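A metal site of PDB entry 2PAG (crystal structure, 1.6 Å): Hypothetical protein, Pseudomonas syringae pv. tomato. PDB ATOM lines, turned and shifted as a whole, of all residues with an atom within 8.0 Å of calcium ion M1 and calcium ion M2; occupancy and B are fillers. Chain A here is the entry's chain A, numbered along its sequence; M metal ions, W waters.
Of the 11 residues printed, 1 comes within 4 Å of calcium ion M2.
Calcium ion M1 is bound by OE1 of Glu 101 (2.1 Å), OG1 of Thr 105 (2.4 Å), OD1 of Asp 103 (2.5 Å) and OD2 of Asp 103 (2.5 Å).
Three residues have an atom within 4 Å of calcium ion M1: Glu 101, Asp 103 and Thr 105.
The nearest printed residue that does not touch calcium ion M1 is Gly 104 (5.6 Å).
Calcium ion M2 is bound by OD2 of Asp 103 (2.4 Å), water W4 (2.4 Å), water W2 (2.5 Å), water W1 (2.6 Å) and water W3 (2.8 Å).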
ATOM      1  N   VAL A 100     -10.468 -22.112  15.649  1.00  0.00           N
ATOM      2  CA  VAL A 100     -11.385 -23.105  16.165  1.00  0.00           C
ATOM      3  C   VAL A 100     -10.953 -24.539  15.882  1.00  0.00           C
ATOM      4  O   VAL A 100     -10.617 -24.889  14.739  1.00  0.00           O
ATOM      5  CB  VAL A 100     -12.779 -22.880  15.591  1.00  0.00           C
ATOM      6  CG1 VAL A 100     -13.807 -23.731  16.327  1.00  0.00           C
ATOM      7  CG2 VAL A 100     -13.136 -21.397  15.710  1.00  0.00           C
ATOM      8  N   GLU A 101     -10.961 -25.350  16.934  1.00  0.00           N
ATOM      9  CA  GLU A 101     -10.597 -26.759  16.838  1.00  0.00           C
ATOM     10  C   GLU A 101     -11.756 -27.500  16.195  1.00  0.00           C
ATOM     11  O   GLU A 101     -12.864 -26.970  16.079  1.00  0.00           O
ATOM     12  CB  GLU A 101     -10.361 -27.356  18.224  1.00  0.00           C
ATOM     13  CG  GLU A 101      -9.176 -26.831  18.994  1.00  0.00           C
ATOM     14  CD  GLU A 101      -8.824 -27.756  20.146  1.00  0.00           C
ATOM     15  OE1 GLU A 101      -9.760 -28.212  20.844  1.00  0.00           O
ATOM     16  OE2 GLU A 101      -7.619 -28.020  20.355  1.00  0.00           O
ATOM     17  N   GLU A 102     -11.501 -28.744  15.785  1.00  0.00           N
ATOM     18  CA  GLU A 102     -12.536 -29.549  15.151  1.00  0.00           C
ATOM     19  C   GLU A 102     -13.736 -29.765  16.072  1.00  0.00           C
ATOM     20  O   GLU A 102     -14.870 -29.856  15.596  1.00  0.00           O
ATOM     21  CB  GLU A 102     -11.934 -30.874  14.691  1.00  0.00           C
ATOM     22  CG  GLU A 102     -10.701 -30.662  13.810  1.00  0.00           C
ATOM     23  CD  GLU A 102     -10.100 -31.957  13.290  1.00  0.00           C
ATOM     24  OE1 GLU A 102     -10.776 -32.657  12.504  1.00  0.00           O
ATOM     25  OE2 GLU A 102      -8.953 -32.271  13.665  1.00  0.00           O
ATOM     26  N   ASP A 103     -13.483 -29.829  17.378  1.00  0.00           N
ATOM     27  CA  ASP A 103     -14.568 -30.021  18.335  1.00  0.00           C
ATOM     28  C   ASP A 103     -15.185 -28.719  18.829  1.00  0.00           C
ATOM     29  O   ASP A 103     -16.019 -28.730  19.748  1.00  0.00           O
ATOM     30  CB  ASP A 103     -14.130 -30.887  19.532  1.00  0.00           C
ATOM     31  CG  ASP A 103     -13.015 -30.262  20.374  1.00  0.00           C
ATOM     32  OD1 ASP A 103     -12.816 -29.032  20.325  1.00  0.00           O
ATOM     33  OD2 ASP A 103     -12.355 -31.012  21.110  1.00  0.00           O
ATOM     34  N   GLY A 104     -14.792 -27.603  18.225  1.00  0.00           N
ATOM     35  CA  GLY A 104     -15.380 -26.329  18.604  1.00  0.00           C
ATOM     36  C   GLY A 104     -14.643 -25.423  19.571  1.00  0.00           C
ATOM     37  O   GLY A 104     -15.011 -24.245  19.686  1.00  0.00           O
ATOM     38  N   THR A 105     -13.630 -25.931  20.250  1.00  0.00           N
ATOM     39  CA  THR A 105     -12.895 -25.092  21.199  1.00  0.00           C
ATOM     40  C   THR A 105     -12.197 -23.957  20.443  1.00  0.00           C
ATOM     41  O   THR A 105     -11.680 -24.171  19.351  1.00  0.00           O
ATOM     42  CB  THR A 105     -11.816 -25.906  21.950  1.00  0.00           C
ATOM     43  OG1 THR A 105     -12.419 -27.061  22.555  1.00  0.00           O
ATOM     44  CG2 THR A 105     -11.163 -25.053  23.045  1.00  0.00           C
ATOM     45  N   VAL A 106     -12.220 -22.756  21.022  1.00  0.00           N
ATOM     46  CA  VAL A 106     -11.553 -21.613  20.402  1.00  0.00           C
ATOM     47  C   VAL A 106     -10.232 -21.408  21.126  1.00  0.00           C
ATOM     48  O   VAL A 106     -10.185 -21.374  22.352  1.00  0.00           O
ATOM     49  CB  VAL A 106     -12.386 -20.319  20.529  1.00  0.00           C
ATOM     50  CG1 VAL A 106     -11.641 -19.160  19.871  1.00  0.00           C
ATOM     51  CG2 VAL A 106     -13.750 -20.509  19.864  1.00  0.00           C
ATOM     52  N   LEU A 107      -9.165 -21.272  20.353  1.00  0.00           N
ATOM     53  CA  LEU A 107      -7.842 -21.091  20.915  1.00  0.00           C
ATOM     54  C   LEU A 107      -7.237 -19.805  20.370  1.00  0.00           C
ATOM     55  O   LEU A 107      -7.728 -19.238  19.399  1.00  0.00           O
ATOM     56  CB  LEU A 107      -6.924 -22.240  20.510  1.00  0.00           C
ATOM     57  CG  LEU A 107      -7.411 -23.674  20.720  1.00  0.00           C
ATOM     58  CD1 LEU A 107      -6.385 -24.652  20.156  1.00  0.00           C
ATOM     59  CD2 LEU A 107      -7.631 -23.940  22.192  1.00  0.00           C
ATOM     60  N   SER A 120      -8.212 -20.255  26.357  1.00  0.00           N
ATOM     61  CA  SER A 120      -9.162 -20.807  25.393  1.00  0.00           C
ATOM     62  C   SER A 120     -10.600 -20.552  25.821  1.00  0.00           C
ATOM     63  O   SER A 120     -10.865 -20.181  26.962  1.00  0.00           O
ATOM     64  CB  SER A 120      -8.935 -22.308  25.214  1.00  0.00           C
ATOM     65  OG  SER A 120      -9.225 -23.012  26.414  1.00  0.00           O
ATOM     66  N   TRP A 121     -11.521 -20.768  24.883  1.00  0.00           N
ATOM     67  CA  TRP A 121     -12.945 -20.559  25.127  1.00  0.00           C
ATOM     68  C   TRP A 121     -13.687 -21.838  24.739  1.00  0.00           C
ATOM     69  O   TRP A 121     -13.375 -22.462  23.721  1.00  0.00           O
ATOM     70  CB  TRP A 121     -13.439 -19.367  24.307  1.00  0.00           C
ATOM     71  CG  TRP A 121     -12.774 -18.090  24.736  1.00  0.00           C
ATOM     72  CD1 TRP A 121     -13.271 -17.171  25.620  1.00  0.00           C
ATOM     73  CD2 TRP A 121     -11.465 -17.653  24.383  1.00  0.00           C
ATOM     74  NE1 TRP A 121     -12.327 -16.182  25.840  1.00  0.00           N
ATOM     75  CE2 TRP A 121     -11.212 -16.454  25.086  1.00  0.00           C
ATOM     76  CE3 TRP A 121     -10.463 -18.153  23.532  1.00  0.00           C
ATOM     77  CZ2 TRP A 121     -10.005 -15.750  24.978  1.00  0.00           C
ATOM     78  CZ3 TRP A 121      -9.267 -17.446  23.416  1.00  0.00           C
ATOM     79  CH2 TRP A 121      -9.045 -16.260  24.143  1.00  0.00           C
ATOM     80  N   GLU A 122     -14.668 -22.227  25.548  1.00  0.00           N
ATOM     81  CA  GLU A 122     -15.423 -23.453  25.321  1.00  0.00           C
ATOM     82  C   GLU A 122     -16.138 -23.554  23.987  1.00  0.00           C
ATOM     83  O   GLU A 122     -16.348 -24.661  23.489  1.00  0.00           O
ATOM     84  CB  GLU A 122     -16.444 -23.674  26.443  1.00  0.00           C
ATOM     85  CG  GLU A 122     -15.855 -23.968  27.814  1.00  0.00           C
ATOM     86  CD  GLU A 122     -15.052 -22.818  28.379  1.00  0.00           C
ATOM     87  OE1 GLU A 122     -15.431 -21.652  28.152  1.00  0.00           O
ATOM     88  OE2 GLU A 122     -14.036 -23.086  29.066  1.00  0.00           O
HETATM   89 CA    CA M   1     -11.152 -29.091  22.158  1.00  0.00          CA
HETATM   90 CA    CA M   2     -11.588 -33.115  21.841  1.00  0.00          CA
HETATM   91  O   HOH W   1      -9.795 -32.601  20.043  1.00  0.00           O
HETATM   92  O   HOH W   2     -12.344 -34.383  19.856  1.00  0.00           O
HETATM   93  O   HOH W   3     -14.267 -33.779  21.502  1.00  0.00           O
HETATM   94  O   HOH W   4     -13.187 -32.676  23.584  1.00  0.00           O
